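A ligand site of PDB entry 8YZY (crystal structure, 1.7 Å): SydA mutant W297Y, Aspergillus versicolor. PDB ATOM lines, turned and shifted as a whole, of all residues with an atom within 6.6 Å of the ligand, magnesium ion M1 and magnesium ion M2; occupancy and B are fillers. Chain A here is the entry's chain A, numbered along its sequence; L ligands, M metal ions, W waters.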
ATOM      1  N   ASP A  94      23.351  29.630 -18.882  1.00  0.00           N
ATOM      2  CA  ASP A  94      22.673  28.647 -19.753  1.00  0.00           C
ATOM      3  C   ASP A  94      22.788  27.255 -19.196  1.00  0.00           C
ATOM      4  O   ASP A  94      21.914  26.417 -19.460  1.00  0.00           O
ATOM      5  CB  ASP A  94      23.310  28.625 -21.179  1.00  0.00           C
ATOM      6  CG  ASP A  94      22.323  28.130 -22.311  1.00  0.00           C
ATOM      7  OD1 ASP A  94      21.265  28.797 -22.519  1.00  0.00           O
ATOM      8  OD2 ASP A  94      22.615  27.110 -23.021  1.00  0.00           O
ATOM      9  N   GLU A  95      23.854  26.973 -18.443  1.00  0.00           N
ATOM     10  CA  GLU A  95      24.075  25.648 -17.869  1.00  0.00           C
ATOM     11  C   GLU A  95      23.670  25.551 -16.411  1.00  0.00           C
ATOM     12  O   GLU A  95      23.128  24.523 -15.999  1.00  0.00           O
ATOM     13  CB  GLU A  95      25.548  25.230 -18.016  1.00  0.00           C
ATOM     14  CG  GLU A  95      25.985  25.150 -19.469  1.00  0.00           C
ATOM     15  CD  GLU A  95      25.367  23.996 -20.235  1.00  0.00           C
ATOM     16  OE1 GLU A  95      24.613  23.190 -19.646  1.00  0.00           O
ATOM     17  OE2 GLU A  95      25.593  23.941 -21.476  1.00  0.00           O
ATOM     18  N   PHE A 151      17.218  37.379 -22.600  1.00  0.00           N
ATOM     19  CA  PHE A 151      17.857  36.075 -22.428  1.00  0.00           C
ATOM     20  C   PHE A 151      17.667  35.530 -21.019  1.00  0.00           C
ATOM     21  O   PHE A 151      17.415  34.327 -20.832  1.00  0.00           O
ATOM     22  CB  PHE A 151      19.352  36.201 -22.755  1.00  0.00           C
ATOM     23  CG  PHE A 151      20.152  35.002 -22.322  1.00  0.00           C
ATOM     24  CD1 PHE A 151      20.147  33.817 -23.071  1.00  0.00           C
ATOM     25  CD2 PHE A 151      20.879  35.039 -21.151  1.00  0.00           C
ATOM     26  CE1 PHE A 151      20.869  32.687 -22.626  1.00  0.00           C
ATOM     27  CE2 PHE A 151      21.611  33.927 -20.700  1.00  0.00           C
ATOM     28  CZ  PHE A 151      21.606  32.742 -21.449  1.00  0.00           C
ATOM     29  N   GLU A 158      11.722  28.998 -20.483  1.00  0.00           N
ATOM     30  CA  GLU A 158      11.839  27.943 -21.508  1.00  0.00           C
ATOM     31  C   GLU A 158      11.186  26.623 -21.131  1.00  0.00           C
ATOM     32  O   GLU A 158      10.390  26.048 -21.894  1.00  0.00           O
ATOM     33  CB  GLU A 158      13.334  27.677 -21.722  1.00  0.00           C
ATOM     34  CG  GLU A 158      13.867  28.015 -23.032  1.00  0.00           C
ATOM     35  CD  GLU A 158      15.320  27.624 -23.132  1.00  0.00           C
ATOM     36  OE1 GLU A 158      16.076  27.811 -22.129  1.00  0.00           O
ATOM     37  OE2 GLU A 158      15.698  27.148 -24.216  1.00  0.00           O
ATOM     38  N   ARG A 177      12.422  31.719 -29.365  1.00  0.00           N
ATOM     39  CA  ARG A 177      13.801  31.641 -29.810  1.00  0.00           C
ATOM     40  C   ARG A 177      14.446  33.021 -29.841  1.00  0.00           C
ATOM     41  O   ARG A 177      15.634  33.153 -29.536  1.00  0.00           O
ATOM     42  CB  ARG A 177      13.882  30.951 -31.191  1.00  0.00           C
ATOM     43  CG  ARG A 177      15.317  30.821 -31.719  1.00  0.00           C
ATOM     44  CD  ARG A 177      16.226  30.184 -30.609  1.00  0.00           C
ATOM     45  NE  ARG A 177      17.428  29.573 -31.142  1.00  0.00           N
ATOM     46  CZ  ARG A 177      18.496  29.277 -30.400  1.00  0.00           C
ATOM     47  NH1 ARG A 177      18.518  29.536 -29.102  1.00  0.00           N
ATOM     48  NH2 ARG A 177      19.558  28.723 -30.981  1.00  0.00           N
ATOM     49  N   THR A 180      15.481  33.509 -26.197  1.00  0.00           N
ATOM     50  CA  THR A 180      16.558  32.677 -25.664  1.00  0.00           C
ATOM     51  C   THR A 180      17.875  32.761 -26.448  1.00  0.00           C
ATOM     52  O   THR A 180      18.927  32.376 -25.915  1.00  0.00           O
ATOM     53  CB  THR A 180      16.139  31.200 -25.638  1.00  0.00           C
ATOM     54  OG1 THR A 180      15.933  30.749 -26.978  1.00  0.00           O
ATOM     55  CG2 THR A 180      14.883  31.033 -24.842  1.00  0.00           C
ATOM     56  N   GLY A 181      17.854  33.251 -27.692  1.00  0.00           N
ATOM     57  CA  GLY A 181      19.019  33.108 -28.534  1.00  0.00           C
ATOM     58  C   GLY A 181      20.141  34.091 -28.307  1.00  0.00           C
ATOM     59  O   GLY A 181      21.252  33.836 -28.762  1.00  0.00           O
ATOM     60  N   PHE A 182      19.869  35.227 -27.666  1.00  0.00           N
ATOM     61  CA  PHE A 182      20.932  36.204 -27.357  1.00  0.00           C
ATOM     62  C   PHE A 182      21.579  36.766 -28.632  1.00  0.00           C
ATOM     63  O   PHE A 182      22.710  37.272 -28.613  1.00  0.00           O
ATOM     64  CB  PHE A 182      21.982  35.561 -26.431  1.00  0.00           C
ATOM     65  CG  PHE A 182      22.745  36.538 -25.603  1.00  0.00           C
ATOM     66  CD1 PHE A 182      22.083  37.401 -24.732  1.00  0.00           C
ATOM     67  CD2 PHE A 182      24.137  36.575 -25.666  1.00  0.00           C
ATOM     68  CE1 PHE A 182      22.812  38.296 -23.937  1.00  0.00           C
ATOM     69  CE2 PHE A 182      24.879  37.474 -24.875  1.00  0.00           C
ATOM     70  CZ  PHE A 182      24.210  38.332 -24.008  1.00  0.00           C
ATOM     71  N   ASP A 217      20.533  32.615 -34.592  1.00  0.00           N
ATOM     72  CA  ASP A 217      19.641  31.715 -33.853  1.00  0.00           C
ATOM     73  C   ASP A 217      19.514  30.369 -34.559  1.00  0.00           C
ATOM     74  O   ASP A 217      19.798  29.294 -33.980  1.00  0.00           O
ATOM     75  CB  ASP A 217      18.237  32.351 -33.743  1.00  0.00           C
ATOM     76  CG  ASP A 217      18.134  33.468 -32.722  1.00  0.00           C
ATOM     77  OD1 ASP A 217      19.033  33.615 -31.866  1.00  0.00           O
ATOM     78  OD2 ASP A 217      17.111  34.198 -32.768  1.00  0.00           O
ATOM     79  N   ASN A 220      22.638  27.994 -34.972  1.00  0.00           N
ATOM     80  CA  ASN A 220      22.830  27.198 -33.769  1.00  0.00           C
ATOM     81  C   ASN A 220      21.770  26.111 -33.657  1.00  0.00           C
ATOM     82  O   ASN A 220      22.065  24.961 -33.281  1.00  0.00           O
ATOM     83  CB  ASN A 220      22.827  28.059 -32.526  1.00  0.00           C
ATOM     84  CG  ASN A 220      22.824  27.201 -31.289  1.00  0.00           C
ATOM     85  OD1 ASN A 220      21.753  26.854 -30.803  1.00  0.00           O
ATOM     86  ND2 ASN A 220      24.009  26.772 -30.816  1.00  0.00           N
ATOM     87  N   ASP A 221      20.502  26.418 -33.971  1.00  0.00           N
ATOM     88  CA  ASP A 221      19.491  25.356 -33.899  1.00  0.00           C
ATOM     89  C   ASP A 221      19.880  24.154 -34.773  1.00  0.00           C
ATOM     90  O   ASP A 221      19.820  23.004 -34.319  1.00  0.00           O
ATOM     91  CB  ASP A 221      18.115  25.895 -34.263  1.00  0.00           C
ATOM     92  CG  ASP A 221      17.535  26.814 -33.168  1.00  0.00           C
ATOM     93  OD1 ASP A 221      17.504  26.403 -31.966  1.00  0.00           O
ATOM     94  OD2 ASP A 221      17.116  27.960 -33.466  1.00  0.00           O
ATOM     95  N   LEU A 223      22.945  23.247 -35.895  1.00  0.00           N
ATOM     96  CA  LEU A 223      24.205  22.599 -35.554  1.00  0.00           C
ATOM     97  C   LEU A 223      24.219  22.054 -34.129  1.00  0.00           C
ATOM     98  O   LEU A 223      25.066  21.232 -33.780  1.00  0.00           O
ATOM     99  CB  LEU A 223      25.360  23.604 -35.715  1.00  0.00           C
ATOM    100  CG  LEU A 223      25.531  24.058 -37.170  1.00  0.00           C
ATOM    101  CD1 LEU A 223      26.601  25.114 -37.288  1.00  0.00           C
ATOM    102  CD2 LEU A 223      25.804  22.842 -38.102  1.00  0.00           C
ATOM    103  N   SER A 224      23.325  22.526 -33.272  1.00  0.00           N
ATOM    104  CA  SER A 224      23.225  21.984 -31.927  1.00  0.00           C
ATOM    105  C   SER A 224      22.066  21.009 -31.815  1.00  0.00           C
ATOM    106  O   SER A 224      21.851  20.480 -30.713  1.00  0.00           O
ATOM    107  CB  SER A 224      23.086  23.114 -30.880  1.00  0.00           C
ATOM    108  OG  SER A 224      21.861  23.834 -31.024  1.00  0.00           O
ATOM    109  N   PHE A 225      21.327  20.750 -32.901  1.00  0.00           N
ATOM    110  CA  PHE A 225      20.276  19.748 -32.783  1.00  0.00           C
ATOM    111  C   PHE A 225      20.817  18.396 -32.332  1.00  0.00           C
ATOM    112  O   PHE A 225      20.120  17.679 -31.603  1.00  0.00           O
ATOM    113  CB  PHE A 225      19.536  19.584 -34.103  1.00  0.00           C
ATOM    114  CG  PHE A 225      18.327  18.710 -33.996  1.00  0.00           C
ATOM    115  CD1 PHE A 225      17.161  19.193 -33.408  1.00  0.00           C
ATOM    116  CD2 PHE A 225      18.337  17.431 -34.492  1.00  0.00           C
ATOM    117  CE1 PHE A 225      16.026  18.393 -33.326  1.00  0.00           C
ATOM    118  CE2 PHE A 225      17.207  16.622 -34.408  1.00  0.00           C
ATOM    119  CZ  PHE A 225      16.050  17.097 -33.826  1.00  0.00           C
ATOM    120  N   LYS A 227      23.402  17.672 -30.207  1.00  0.00           N
ATOM    121  CA  LYS A 227      23.667  17.581 -28.778  1.00  0.00           C
ATOM    122  C   LYS A 227      22.402  17.795 -27.960  1.00  0.00           C
ATOM    123  O   LYS A 227      22.274  17.252 -26.853  1.00  0.00           O
ATOM    124  CB  LYS A 227      24.787  18.549 -28.354  1.00  0.00           C
ATOM    125  CG  LYS A 227      24.422  20.078 -28.359  1.00  0.00           C
ATOM    126  CD  LYS A 227      24.013  20.562 -26.945  1.00  0.00           C
ATOM    127  CE  LYS A 227      23.904  22.088 -26.949  1.00  0.00           C
ATOM    128  NZ  LYS A 227      23.415  22.564 -25.593  1.00  0.00           N
ATOM    129  N   GLU A 228      21.441  18.556 -28.494  1.00  0.00           N
ATOM    130  CA  GLU A 228      20.232  18.821 -27.712  1.00  0.00           C
ATOM    131  C   GLU A 228      19.265  17.645 -27.790  1.00  0.00           C
ATOM    132  O   GLU A 228      18.780  17.162 -26.756  1.00  0.00           O
ATOM    133  CB  GLU A 228      19.554  20.099 -28.234  1.00  0.00           C
ATOM    134  CG  GLU A 228      20.378  21.300 -27.903  1.00  0.00           C
ATOM    135  CD  GLU A 228      19.950  22.564 -28.579  1.00  0.00           C
ATOM    136  OE1 GLU A 228      18.991  22.559 -29.399  1.00  0.00           O
ATOM    137  OE2 GLU A 228      20.601  23.591 -28.284  1.00  0.00           O
ATOM    138  N   GLU A 234      16.782  17.391 -24.699  1.00  0.00           N
ATOM    139  CA  GLU A 234      16.085  18.671 -24.859  1.00  0.00           C
ATOM    140  C   GLU A 234      14.982  18.544 -25.906  1.00  0.00           C
ATOM    141  O   GLU A 234      15.247  18.147 -27.045  1.00  0.00           O
ATOM    142  CB  GLU A 234      17.079  19.782 -25.220  1.00  0.00           C
ATOM    143  CG  GLU A 234      16.510  21.227 -25.174  1.00  0.00           C
ATOM    144  CD  GLU A 234      17.586  22.332 -25.288  1.00  0.00           C
ATOM    145  OE1 GLU A 234      18.758  22.075 -24.914  1.00  0.00           O
ATOM    146  OE2 GLU A 234      17.260  23.470 -25.776  1.00  0.00           O
ATOM    147  N   ASN A 237      13.456  23.023 -27.523  1.00  0.00           N
ATOM    148  CA  ASN A 237      14.173  23.940 -28.391  1.00  0.00           C
ATOM    149  C   ASN A 237      13.292  24.353 -29.568  1.00  0.00           C
ATOM    150  O   ASN A 237      12.158  23.881 -29.751  1.00  0.00           O
ATOM    151  CB  ASN A 237      15.500  23.336 -28.826  1.00  0.00           C
ATOM    152  CG  ASN A 237      15.336  21.962 -29.485  1.00  0.00           C
ATOM    153  OD1 ASN A 237      14.244  21.599 -29.922  1.00  0.00           O
ATOM    154  ND2 ASN A 237      16.410  21.202 -29.513  1.00  0.00           N
ATOM    155  N   HIS A 293      31.045  25.908 -34.011  1.00  0.00           N
ATOM    156  CA  HIS A 293      30.194  24.771 -33.658  1.00  0.00           C
ATOM    157  C   HIS A 293      30.868  23.439 -33.977  1.00  0.00           C
ATOM    158  O   HIS A 293      30.712  22.459 -33.241  1.00  0.00           O
ATOM    159  CB  HIS A 293      28.858  24.850 -34.388  1.00  0.00           C
ATOM    160  CG  HIS A 293      27.926  25.840 -33.782  1.00  0.00           C
ATOM    161  ND1 HIS A 293      28.027  27.193 -34.035  1.00  0.00           N
ATOM    162  CD2 HIS A 293      26.861  25.696 -32.953  1.00  0.00           C
ATOM    163  CE1 HIS A 293      27.080  27.843 -33.349  1.00  0.00           C
ATOM    164  NE2 HIS A 293      26.354  26.954 -32.696  1.00  0.00           N
ATOM    165  N   ARG A 299      31.090  20.868 -26.559  1.00  0.00           N
ATOM    166  CA  ARG A 299      29.747  21.417 -26.414  1.00  0.00           C
ATOM    167  C   ARG A 299      28.750  20.847 -27.426  1.00  0.00           C
ATOM    168  O   ARG A 299      27.601  20.571 -27.044  1.00  0.00           O
ATOM    169  CB  ARG A 299      29.798  22.957 -26.521  1.00  0.00           C
ATOM    170  CG  ARG A 299      28.515  23.612 -26.059  1.00  0.00           C
ATOM    171  CD  ARG A 299      28.499  25.155 -26.123  1.00  0.00           C
ATOM    172  NE  ARG A 299      27.212  25.645 -25.631  1.00  0.00           N
ATOM    173  CZ  ARG A 299      26.808  25.585 -24.369  1.00  0.00           C
ATOM    174  NH1 ARG A 299      27.625  25.184 -23.406  1.00  0.00           N
ATOM    175  NH2 ARG A 299      25.558  25.899 -24.078  1.00  0.00           N
ATOM    176  N   TYR A 300      29.163  20.603 -28.685  1.00  0.00           N
ATOM    177  CA  TYR A 300      28.243  20.162 -29.741  1.00  0.00           C
ATOM    178  C   TYR A 300      28.503  18.759 -30.252  1.00  0.00           C
ATOM    179  O   TYR A 300      27.635  18.205 -30.941  1.00  0.00           O
ATOM    180  CB  TYR A 300      28.269  21.133 -30.940  1.00  0.00           C
ATOM    181  CG  TYR A 300      27.941  22.524 -30.436  1.00  0.00           C
ATOM    182  CD1 TYR A 300      26.674  22.821 -29.968  1.00  0.00           C
ATOM    183  CD2 TYR A 300      28.934  23.521 -30.344  1.00  0.00           C
ATOM    184  CE1 TYR A 300      26.369  24.101 -29.451  1.00  0.00           C
ATOM    185  CE2 TYR A 300      28.638  24.815 -29.833  1.00  0.00           C
ATOM    186  CZ  TYR A 300      27.356  25.085 -29.398  1.00  0.00           C
ATOM    187  OH  TYR A 300      27.029  26.319 -28.882  1.00  0.00           O
HETATM  188  P1  LIG L   1      23.509  26.019 -27.322  1.00  0.00           P
HETATM  189  O1  LIG L   1      23.083  25.390 -26.009  1.00  0.00           O
HETATM  190  O2  LIG L   1      23.080  25.264 -28.543  1.00  0.00           O
HETATM  191  O3  LIG L   1      24.951  26.361 -27.399  1.00  0.00           O
HETATM  192  O4  LIG L   1      22.743  27.463 -27.347  1.00  0.00           O
HETATM  193  P2  LIG L   1      21.149  27.608 -27.147  1.00  0.00           P
HETATM  194  O5  LIG L   1      20.467  26.664 -28.078  1.00  0.00           O
HETATM  195  O6  LIG L   1      20.804  27.338 -25.713  1.00  0.00           O
HETATM  196  O7  LIG L   1      20.843  29.044 -27.503  1.00  0.00           O
HETATM  197 MG    MG M   1      21.479  25.711 -24.590  1.00  0.00          MG
HETATM  198 MG    MG M   2      21.195  25.321 -29.427  1.00  0.00          MG
HETATM  199  O   HOH W   1      17.896  26.070 -27.526  1.00  0.00           O
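The nearest printed residue that does not touch the ligand is Thr 180 (4.2 Å).
OD1 of Asn 220 sits close to NH2 of Arg 177, at 2.9 Å.
O of Glu 228 sits at hydrogen-bond distance from N of Glu 234, at 2.9 Å.
The guanidinium group (NE) of Arg 177 is in salt-bridge range of the side-chain carboxylate (OD2) of Asp 221 (2.8 Å).
ND2 of Asn 237 is in hydrogen-bond range of OE1 of Glu 228 (2.9 Å).
NE2 of His 293 sits at hydrogen-bond distance from ND2 of Asn 220.
The guanidinium group of Arg 299 lies within salt-bridge range of the side-chain carboxylate of Glu 95.
NE of Arg 299 sits at hydrogen-bond distance from OH of Tyr 300 (3.3 Å).
OD2 of Asp 94 lies close to NH2 of Arg 299, at 3.4 Å.
Magnesium ion M2 is bound by an oxygen (O5) of the ligand, an oxygen (O2) of the ligand, the side-chain amide oxygen of Asn 220, the side-chain carboxylate of Glu 228 and the side-chain hydroxyl of Ser 224.
Lys 227 touches magnesium ion M1.
The guanidinium group (NH1) of Arg 177 lies within salt-bridge range of an oxygen (O7) of the ligand, 2.9 Å away.
An oxygen (O3) of the ligand is in salt-bridge range of the guanidinium group of Arg 299 (3.0 Å).
OH of Tyr 300 sits at hydrogen-bond distance from O3 of the ligand (2.6 Å).
NZ of Lys 227 lies close to O1 of the ligand (2.9 Å).
Magnesium ion M1 is bound by an oxygen (O6) of the ligand (2.1 Å), an oxygen (O1) of the ligand (2.2 Å) and the side-chain carboxylate of Asp 94 (2.4 Å).
Within 4 Å of magnesium ion M2: Asn 220, Ser 224 and Glu 228.
Along chain A the residues within 4 Å of magnesium ion M2 span positions 220 to 228.
The nearest printed residue that does not touch magnesium ion M2 is Arg 177 (4.1 Å).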
